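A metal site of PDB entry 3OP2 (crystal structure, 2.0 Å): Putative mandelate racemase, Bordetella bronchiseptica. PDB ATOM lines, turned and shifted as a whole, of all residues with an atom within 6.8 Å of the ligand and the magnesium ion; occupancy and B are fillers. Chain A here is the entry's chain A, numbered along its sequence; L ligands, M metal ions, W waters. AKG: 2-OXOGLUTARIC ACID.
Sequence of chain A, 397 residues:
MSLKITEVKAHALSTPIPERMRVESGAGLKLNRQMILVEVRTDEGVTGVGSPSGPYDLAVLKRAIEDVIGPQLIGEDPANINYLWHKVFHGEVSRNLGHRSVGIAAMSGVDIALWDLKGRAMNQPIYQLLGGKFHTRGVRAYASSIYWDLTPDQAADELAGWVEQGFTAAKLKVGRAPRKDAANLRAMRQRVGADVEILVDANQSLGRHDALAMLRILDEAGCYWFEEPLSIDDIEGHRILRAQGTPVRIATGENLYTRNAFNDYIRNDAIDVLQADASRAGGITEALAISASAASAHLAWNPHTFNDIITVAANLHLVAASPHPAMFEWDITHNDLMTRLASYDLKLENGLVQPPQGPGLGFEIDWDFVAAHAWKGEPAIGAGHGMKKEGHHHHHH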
ATOM      1  N   GLU A  24      24.155  22.706  16.251  1.00  0.00           N
ATOM      2  CA  GLU A  24      24.798  23.615  15.291  1.00  0.00           C
ATOM      3  C   GLU A  24      25.704  24.681  15.953  1.00  0.00           C
ATOM      4  O   GLU A  24      26.796  24.952  15.462  1.00  0.00           O
ATOM      5  CB  GLU A  24      23.758  24.243  14.353  1.00  0.00           C
ATOM      6  CG  GLU A  24      23.035  23.191  13.489  1.00  0.00           C
ATOM      7  CD  GLU A  24      22.100  23.774  12.429  1.00  0.00           C
ATOM      8  OE1 GLU A  24      21.444  24.807  12.696  1.00  0.00           O
ATOM      9  OE2 GLU A  24      22.019  23.194  11.324  1.00  0.00           O
ATOM     10  N   LYS A  30      22.454  16.567  20.469  1.00  0.00           N
ATOM     11  CA  LYS A  30      21.119  16.180  20.031  1.00  0.00           C
ATOM     12  C   LYS A  30      20.822  14.795  20.589  1.00  0.00           C
ATOM     13  O   LYS A  30      21.381  13.795  20.145  1.00  0.00           O
ATOM     14  CB  LYS A  30      21.066  16.169  18.509  1.00  0.00           C
ATOM     15  CG  LYS A  30      21.254  17.512  17.858  1.00  0.00           C
ATOM     16  CD  LYS A  30      21.806  17.339  16.453  1.00  0.00           C
ATOM     17  CE  LYS A  30      21.865  18.670  15.708  1.00  0.00           C
ATOM     18  NZ  LYS A  30      22.645  18.587  14.428  1.00  0.00           N
ATOM     19  N   ARG A  33      14.930  12.194  19.288  1.00  0.00           N
ATOM     20  CA  ARG A  33      13.917  12.681  18.353  1.00  0.00           C
ATOM     21  C   ARG A  33      12.579  12.589  19.068  1.00  0.00           C
ATOM     22  O   ARG A  33      12.268  11.567  19.707  1.00  0.00           O
ATOM     23  CB  ARG A  33      13.914  11.856  17.069  1.00  0.00           C
ATOM     24  CG  ARG A  33      15.301  11.612  16.520  1.00  0.00           C
ATOM     25  CD  ARG A  33      15.316  11.309  15.044  1.00  0.00           C
ATOM     26  NE  ARG A  33      15.144  12.506  14.221  1.00  0.00           N
ATOM     27  CZ  ARG A  33      16.150  13.275  13.794  1.00  0.00           C
ATOM     28  NH1 ARG A  33      17.408  12.984  14.106  1.00  0.00           N
ATOM     29  NH2 ARG A  33      15.890  14.348  13.048  1.00  0.00           N
ATOM     30  N   TYR A 142      13.024  16.404  -2.974  1.00  0.00           N
ATOM     31  CA  TYR A 142      14.430  16.741  -2.786  1.00  0.00           C
ATOM     32  C   TYR A 142      14.978  16.156  -1.485  1.00  0.00           C
ATOM     33  O   TYR A 142      14.218  15.967  -0.511  1.00  0.00           O
ATOM     34  CB  TYR A 142      14.694  18.252  -2.928  1.00  0.00           C
ATOM     35  CG  TYR A 142      14.238  19.120  -1.789  1.00  0.00           C
ATOM     36  CD1 TYR A 142      15.082  19.379  -0.709  1.00  0.00           C
ATOM     37  CD2 TYR A 142      12.974  19.711  -1.791  1.00  0.00           C
ATOM     38  CE1 TYR A 142      14.682  20.186   0.352  1.00  0.00           C
ATOM     39  CE2 TYR A 142      12.556  20.534  -0.734  1.00  0.00           C
ATOM     40  CZ  TYR A 142      13.427  20.768   0.325  1.00  0.00           C
ATOM     41  OH  TYR A 142      13.035  21.561   1.393  1.00  0.00           O
ATOM     42  N   SER A 144      16.905  16.347   1.876  1.00  0.00           N
ATOM     43  CA  SER A 144      17.208  17.375   2.875  1.00  0.00           C
ATOM     44  C   SER A 144      17.850  16.790   4.144  1.00  0.00           C
ATOM     45  O   SER A 144      17.240  15.964   4.833  1.00  0.00           O
ATOM     46  CB  SER A 144      15.938  18.128   3.254  1.00  0.00           C
ATOM     47  OG  SER A 144      16.203  19.097   4.261  1.00  0.00           O
ATOM     48  N   SER A 145      19.073  17.209   4.478  1.00  0.00           N
ATOM     49  CA  SER A 145      19.843  18.199   3.722  1.00  0.00           C
ATOM     50  C   SER A 145      21.337  17.931   3.916  1.00  0.00           C
ATOM     51  O   SER A 145      21.734  17.240   4.849  1.00  0.00           O
ATOM     52  CB  SER A 145      19.516  19.636   4.178  1.00  0.00           C
ATOM     53  OG  SER A 145      19.563  19.758   5.589  1.00  0.00           O
ATOM     54  N   TYR A 147      24.876  19.002   5.082  1.00  0.00           N
ATOM     55  CA  TYR A 147      25.461  19.888   6.092  1.00  0.00           C
ATOM     56  C   TYR A 147      26.508  20.831   5.476  1.00  0.00           C
ATOM     57  O   TYR A 147      27.167  20.487   4.490  1.00  0.00           O
ATOM     58  CB  TYR A 147      26.086  19.058   7.213  1.00  0.00           C
ATOM     59  CG  TYR A 147      26.261  19.807   8.510  1.00  0.00           C
ATOM     60  CD1 TYR A 147      25.164  20.221   9.263  1.00  0.00           C
ATOM     61  CD2 TYR A 147      27.541  20.084   9.000  1.00  0.00           C
ATOM     62  CE1 TYR A 147      25.323  20.891  10.472  1.00  0.00           C
ATOM     63  CE2 TYR A 147      27.711  20.760  10.203  1.00  0.00           C
ATOM     64  CZ  TYR A 147      26.607  21.159  10.927  1.00  0.00           C
ATOM     65  OH  TYR A 147      26.782  21.821  12.129  1.00  0.00           O
ATOM     66  N   LYS A 171      19.113  19.753  -1.098  1.00  0.00           N
ATOM     67  CA  LYS A 171      19.330  21.037  -0.398  1.00  0.00           C
ATOM     68  C   LYS A 171      20.623  21.051   0.424  1.00  0.00           C
ATOM     69  O   LYS A 171      20.918  20.096   1.171  1.00  0.00           O
ATOM     70  CB  LYS A 171      18.127  21.366   0.481  1.00  0.00           C
ATOM     71  CG  LYS A 171      18.104  22.775   1.065  1.00  0.00           C
ATOM     72  CD  LYS A 171      16.694  23.129   1.521  1.00  0.00           C
ATOM     73  CE  LYS A 171      16.392  22.534   2.886  1.00  0.00           C
ATOM     74  NZ  LYS A 171      14.974  22.729   3.308  1.00  0.00           N
ATOM     75  N   LYS A 173      22.934  23.258   3.263  1.00  0.00           N
ATOM     76  CA  LYS A 173      23.058  24.296   4.277  1.00  0.00           C
ATOM     77  C   LYS A 173      24.212  25.222   3.931  1.00  0.00           C
ATOM     78  O   LYS A 173      25.276  24.771   3.503  1.00  0.00           O
ATOM     79  CB  LYS A 173      23.223  23.698   5.673  1.00  0.00           C
ATOM     80  CG  LYS A 173      21.912  23.221   6.280  1.00  0.00           C
ATOM     81  CD  LYS A 173      22.107  22.584   7.653  1.00  0.00           C
ATOM     82  CE  LYS A 173      20.797  22.431   8.391  1.00  0.00           C
ATOM     83  NZ  LYS A 173      19.804  21.618   7.628  1.00  0.00           N
ATOM     84  N   ASP A 201      19.914  26.551   1.954  1.00  0.00           N
ATOM     85  CA  ASP A 201      19.169  26.966   3.162  1.00  0.00           C
ATOM     86  C   ASP A 201      20.126  27.681   4.120  1.00  0.00           C
ATOM     87  O   ASP A 201      21.114  27.079   4.576  1.00  0.00           O
ATOM     88  CB  ASP A 201      18.521  25.739   3.861  1.00  0.00           C
ATOM     89  CG  ASP A 201      17.517  26.113   4.957  1.00  0.00           C
ATOM     90  OD1 ASP A 201      17.604  27.193   5.590  1.00  0.00           O
ATOM     91  OD2 ASP A 201      16.619  25.276   5.216  1.00  0.00           O
ATOM     92  N   ALA A 202      19.848  28.944   4.418  1.00  0.00           N
ATOM     93  CA  ALA A 202      20.768  29.736   5.258  1.00  0.00           C
ATOM     94  C   ALA A 202      20.354  29.769   6.727  1.00  0.00           C
ATOM     95  O   ALA A 202      21.097  30.248   7.570  1.00  0.00           O
ATOM     96  CB  ALA A 202      20.941  31.152   4.711  1.00  0.00           C
ATOM     97  N   ASN A 203      19.166  29.262   7.016  1.00  0.00           N
ATOM     98  CA  ASN A 203      18.638  29.184   8.376  1.00  0.00           C
ATOM     99  C   ASN A 203      18.668  30.527   9.102  1.00  0.00           C
ATOM    100  O   ASN A 203      18.980  30.582  10.288  1.00  0.00           O
ATOM    101  CB  ASN A 203      19.342  28.067   9.176  1.00  0.00           C
ATOM    102  CG  ASN A 203      19.045  26.683   8.626  1.00  0.00           C
ATOM    103  OD1 ASN A 203      19.874  26.082   7.935  1.00  0.00           O
ATOM    104  ND2 ASN A 203      17.844  26.188   8.899  1.00  0.00           N
ATOM    105  N   GLU A 227      16.740  29.635   0.721  1.00  0.00           N
ATOM    106  CA  GLU A 227      15.789  29.429   1.825  1.00  0.00           C
ATOM    107  C   GLU A 227      16.241  30.120   3.110  1.00  0.00           C
ATOM    108  O   GLU A 227      17.441  30.100   3.449  1.00  0.00           O
ATOM    109  CB  GLU A 227      15.571  27.908   2.057  1.00  0.00           C
ATOM    110  CG  GLU A 227      14.612  27.542   3.215  1.00  0.00           C
ATOM    111  CD  GLU A 227      14.261  26.048   3.275  1.00  0.00           C
ATOM    112  OE1 GLU A 227      14.396  25.336   2.264  1.00  0.00           O
ATOM    113  OE2 GLU A 227      13.817  25.589   4.347  1.00  0.00           O
ATOM    114  N   GLU A 228      15.290  30.728   3.812  1.00  0.00           N
ATOM    115  CA  GLU A 228      15.571  31.552   4.993  1.00  0.00           C
ATOM    116  C   GLU A 228      16.906  32.316   4.891  1.00  0.00           C
ATOM    117  O   GLU A 228      17.835  32.096   5.688  1.00  0.00           O
ATOM    118  CB  GLU A 228      15.511  30.713   6.280  1.00  0.00           C
ATOM    119  CG  GLU A 228      14.113  30.142   6.601  1.00  0.00           C
ATOM    120  CD  GLU A 228      13.993  29.692   8.054  1.00  0.00           C
ATOM    121  OE1 GLU A 228      14.851  28.904   8.531  1.00  0.00           O
ATOM    122  OE2 GLU A 228      13.034  30.111   8.733  1.00  0.00           O
ATOM    123  N   GLU A 254       9.036  27.958   7.100  1.00  0.00           N
ATOM    124  CA  GLU A 254       8.949  26.908   8.122  1.00  0.00           C
ATOM    125  C   GLU A 254       8.726  27.455   9.530  1.00  0.00           C
ATOM    126  O   GLU A 254       8.186  26.761  10.402  1.00  0.00           O
ATOM    127  CB  GLU A 254      10.175  26.006   8.087  1.00  0.00           C
ATOM    128  CG  GLU A 254      11.426  26.688   8.574  1.00  0.00           C
ATOM    129  CD  GLU A 254      12.662  25.891   8.333  1.00  0.00           C
ATOM    130  OE1 GLU A 254      13.214  25.378   9.311  1.00  0.00           O
ATOM    131  OE2 GLU A 254      13.097  25.783   7.165  1.00  0.00           O
ATOM    132  N   ASN A 255       9.147  28.706   9.744  1.00  0.00           N
ATOM    133  CA  ASN A 255       9.015  29.377  11.029  1.00  0.00           C
ATOM    134  C   ASN A 255       7.931  30.466  11.070  1.00  0.00           C
ATOM    135  O   ASN A 255       7.867  31.247  12.024  1.00  0.00           O
ATOM    136  CB  ASN A 255      10.374  29.939  11.461  1.00  0.00           C
ATOM    137  CG  ASN A 255      11.369  28.852  11.822  1.00  0.00           C
ATOM    138  OD1 ASN A 255      12.512  28.852  11.341  1.00  0.00           O
ATOM    139  ND2 ASN A 255      10.956  27.926  12.667  1.00  0.00           N
ATOM    140  N   GLN A 275       6.736  28.289   2.363  1.00  0.00           N
ATOM    141  CA  GLN A 275       7.110  26.981   2.891  1.00  0.00           C
ATOM    142  C   GLN A 275       6.374  26.641   4.178  1.00  0.00           C
ATOM    143  O   GLN A 275       6.866  25.840   4.985  1.00  0.00           O
ATOM    144  CB  GLN A 275       8.613  26.924   3.116  1.00  0.00           C
ATOM    145  CG  GLN A 275       9.430  27.103   1.843  1.00  0.00           C
ATOM    146  CD  GLN A 275      10.918  27.046   2.086  1.00  0.00           C
ATOM    147  OE1 GLN A 275      11.465  27.907   2.762  1.00  0.00           O
ATOM    148  NE2 GLN A 275      11.579  26.036   1.530  1.00  0.00           N
ATOM    149  N   HIS A 304       7.703  23.101   4.118  1.00  0.00           N
ATOM    150  CA  HIS A 304       8.610  22.407   5.019  1.00  0.00           C
ATOM    151  C   HIS A 304       7.825  21.230   5.592  1.00  0.00           C
ATOM    152  O   HIS A 304       6.664  21.411   5.964  1.00  0.00           O
ATOM    153  CB  HIS A 304       8.996  23.361   6.127  1.00  0.00           C
ATOM    154  CG  HIS A 304       9.730  22.720   7.257  1.00  0.00           C
ATOM    155  ND1 HIS A 304       9.086  22.095   8.306  1.00  0.00           N
ATOM    156  CD2 HIS A 304      11.060  22.620   7.519  1.00  0.00           C
ATOM    157  CE1 HIS A 304       9.982  21.637   9.159  1.00  0.00           C
ATOM    158  NE2 HIS A 304      11.183  21.949   8.706  1.00  0.00           N
ATOM    159  N   THR A 305       8.435  20.048   5.668  1.00  0.00           N
ATOM    160  CA  THR A 305       7.721  18.819   6.079  1.00  0.00           C
ATOM    161  C   THR A 305       8.379  18.076   7.259  1.00  0.00           C
ATOM    162  O   THR A 305       7.832  17.103   7.793  1.00  0.00           O
ATOM    163  CB  THR A 305       7.588  17.805   4.904  1.00  0.00           C
ATOM    164  OG1 THR A 305       8.863  17.215   4.627  1.00  0.00           O
ATOM    165  CG2 THR A 305       7.044  18.471   3.632  1.00  0.00           C
ATOM    166  N   PHE A 306       9.554  18.561   7.656  1.00  0.00           N
ATOM    167  CA  PHE A 306      10.553  17.902   8.482  1.00  0.00           C
ATOM    168  C   PHE A 306      10.146  17.725   9.955  1.00  0.00           C
ATOM    169  O   PHE A 306      10.166  18.696  10.722  1.00  0.00           O
ATOM    170  CB  PHE A 306      11.804  18.801   8.390  1.00  0.00           C
ATOM    171  CG  PHE A 306      13.100  18.168   8.818  1.00  0.00           C
ATOM    172  CD1 PHE A 306      13.375  17.911  10.164  1.00  0.00           C
ATOM    173  CD2 PHE A 306      14.104  17.904   7.872  1.00  0.00           C
ATOM    174  CE1 PHE A 306      14.601  17.364  10.554  1.00  0.00           C
ATOM    175  CE2 PHE A 306      15.339  17.340   8.248  1.00  0.00           C
ATOM    176  CZ  PHE A 306      15.593  17.081   9.603  1.00  0.00           C
ATOM    177  N   GLU A 329      10.164  18.388   0.268  1.00  0.00           N
ATOM    178  CA  GLU A 329      11.220  18.096   1.219  1.00  0.00           C
ATOM    179  C   GLU A 329      11.137  16.676   1.759  1.00  0.00           C
ATOM    180  O   GLU A 329      10.120  16.290   2.362  1.00  0.00           O
ATOM    181  CB  GLU A 329      11.182  19.097   2.373  1.00  0.00           C
ATOM    182  CG  GLU A 329      12.280  18.858   3.391  1.00  0.00           C
ATOM    183  CD  GLU A 329      12.378  19.926   4.448  1.00  0.00           C
ATOM    184  OE1 GLU A 329      11.325  20.422   4.903  1.00  0.00           O
ATOM    185  OE2 GLU A 329      13.515  20.257   4.824  1.00  0.00           O
ATOM    186  N   THR A 333      17.776  12.220   6.992  1.00  0.00           N
ATOM    187  CA  THR A 333      18.530  11.828   8.192  1.00  0.00           C
ATOM    188  C   THR A 333      17.919  10.603   8.863  1.00  0.00           C
ATOM    189  O   THR A 333      16.736  10.286   8.672  1.00  0.00           O
ATOM    190  CB  THR A 333      18.632  12.982   9.244  1.00  0.00           C
ATOM    191  OG1 THR A 333      17.369  13.184   9.881  1.00  0.00           O
ATOM    192  CG2 THR A 333      19.122  14.273   8.603  1.00  0.00           C
HETATM  193  C1  AKG L   1      14.750  22.460   7.028  1.00  0.00           C
HETATM  194  O1  AKG L   1      14.313  21.293   7.125  1.00  0.00           O
HETATM  195  O2  AKG L   1      14.431  23.214   6.068  1.00  0.00           O
HETATM  196  C2  AKG L   1      15.617  22.998   8.066  1.00  0.00           C
HETATM  197  O5  AKG L   1      15.992  24.166   7.964  1.00  0.00           O
HETATM  198  C3  AKG L   1      16.033  22.194   9.281  1.00  0.00           C
HETATM  199  C4  AKG L   1      16.885  20.982   8.899  1.00  0.00           C
HETATM  200  C5  AKG L   1      17.766  20.505  10.045  1.00  0.00           C
HETATM  201  O3  AKG L   1      17.312  20.433  11.207  1.00  0.00           O
HETATM  202  O4  AKG L   1      18.940  20.156   9.783  1.00  0.00           O
HETATM  203 MG    MG M   1      14.720  25.312   6.201  1.00  0.00          MG
HETATM  204  O   HOH W   1      13.018  22.020  10.939  1.00  0.00           O
HETATM  205  O   HOH W   2      15.401  27.206   6.921  1.00  0.00           O
HETATM  206  O   HOH W   3      11.856  23.686   4.269  1.00  0.00           O
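OE2 of Glu 329 sits close to O1 of the ligand (2.6 Å). NZ of Lys 173 is in salt-bridge range of O4 of the ligand (2.7 Å). The side-chain amino group of Lys 171 sits close to an oxygen (O2) of the ligand. The side-chain amide nitrogen of Asn 203 lies close to an oxygen (O5) of the ligand (2.9 Å).
OE1 of Glu 227 is in salt-bridge range of NZ of Lys 171 (2.9 Å). The side-chain carboxylate of Glu 227 is in hydrogen-bond range of the side-chain amide nitrogen of Gln 275, 3.0 Å away. The backbone carbonyl oxygen (O) of Glu 227 is in hydrogen-bond range of the backbone NH (N) of Ala 202 (2.8 Å). The side-chain carboxylate of Asp 201 is in hydrogen-bond range of the backbone NH of Asn 203, 3.0 Å away. OE2 of Glu 329 lies within salt-bridge range of NZ of Lys 171, 3.2 Å away. The side-chain amino group (NZ) of Lys 171 is in hydrogen-bond range of the side-chain hydroxyl (OH) of Tyr 142 (3.0 Å). N of Asn 203 lies within hydrogen-bond range of O of Glu 228, at 3.4 Å. The backbone NH of His 304 is in hydrogen-bond range of the backbone carbonyl oxygen of Gln 275 (3.0 Å).
His 304 touches the ligand. Phe 306 touches the ligand. Hydrophobic or aromatic side chains within 4 Å of the ligand: His 304 and Phe 306.
Residues that only touch the magnesium ion: Lys 171 (3.9 Å). Of the 22 residues printed, 4 come within 4 Å of the magnesium ion. Along chain A the residues within 4 Å of the magnesium ion span positions 171 to 254. The nearest printed residue that does not touch the magnesium ion is Asn 203 (4.2 Å).
The magnesium ion is bound by OE2 of Glu 254 (1.9 Å), OE2 of Glu 227 (2.1 Å), O2 of the ligand (2.1 Å), water W2 (2.1 Å), OD2 of Asp 201 (2.1 Å) and O5 of the ligand (2.5 Å).
Water W2 lies within hydrogen-bond range of the side-chain carboxylate of Glu 228 (2.4 Å), the side-chain carboxylate of Asp 201 (2.6 Å) and the side-chain amide nitrogen of Asn 203 (3.3 Å). Water W3 lies within hydrogen-bond range of OE1 of Glu 329 and NZ of Lys 171.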
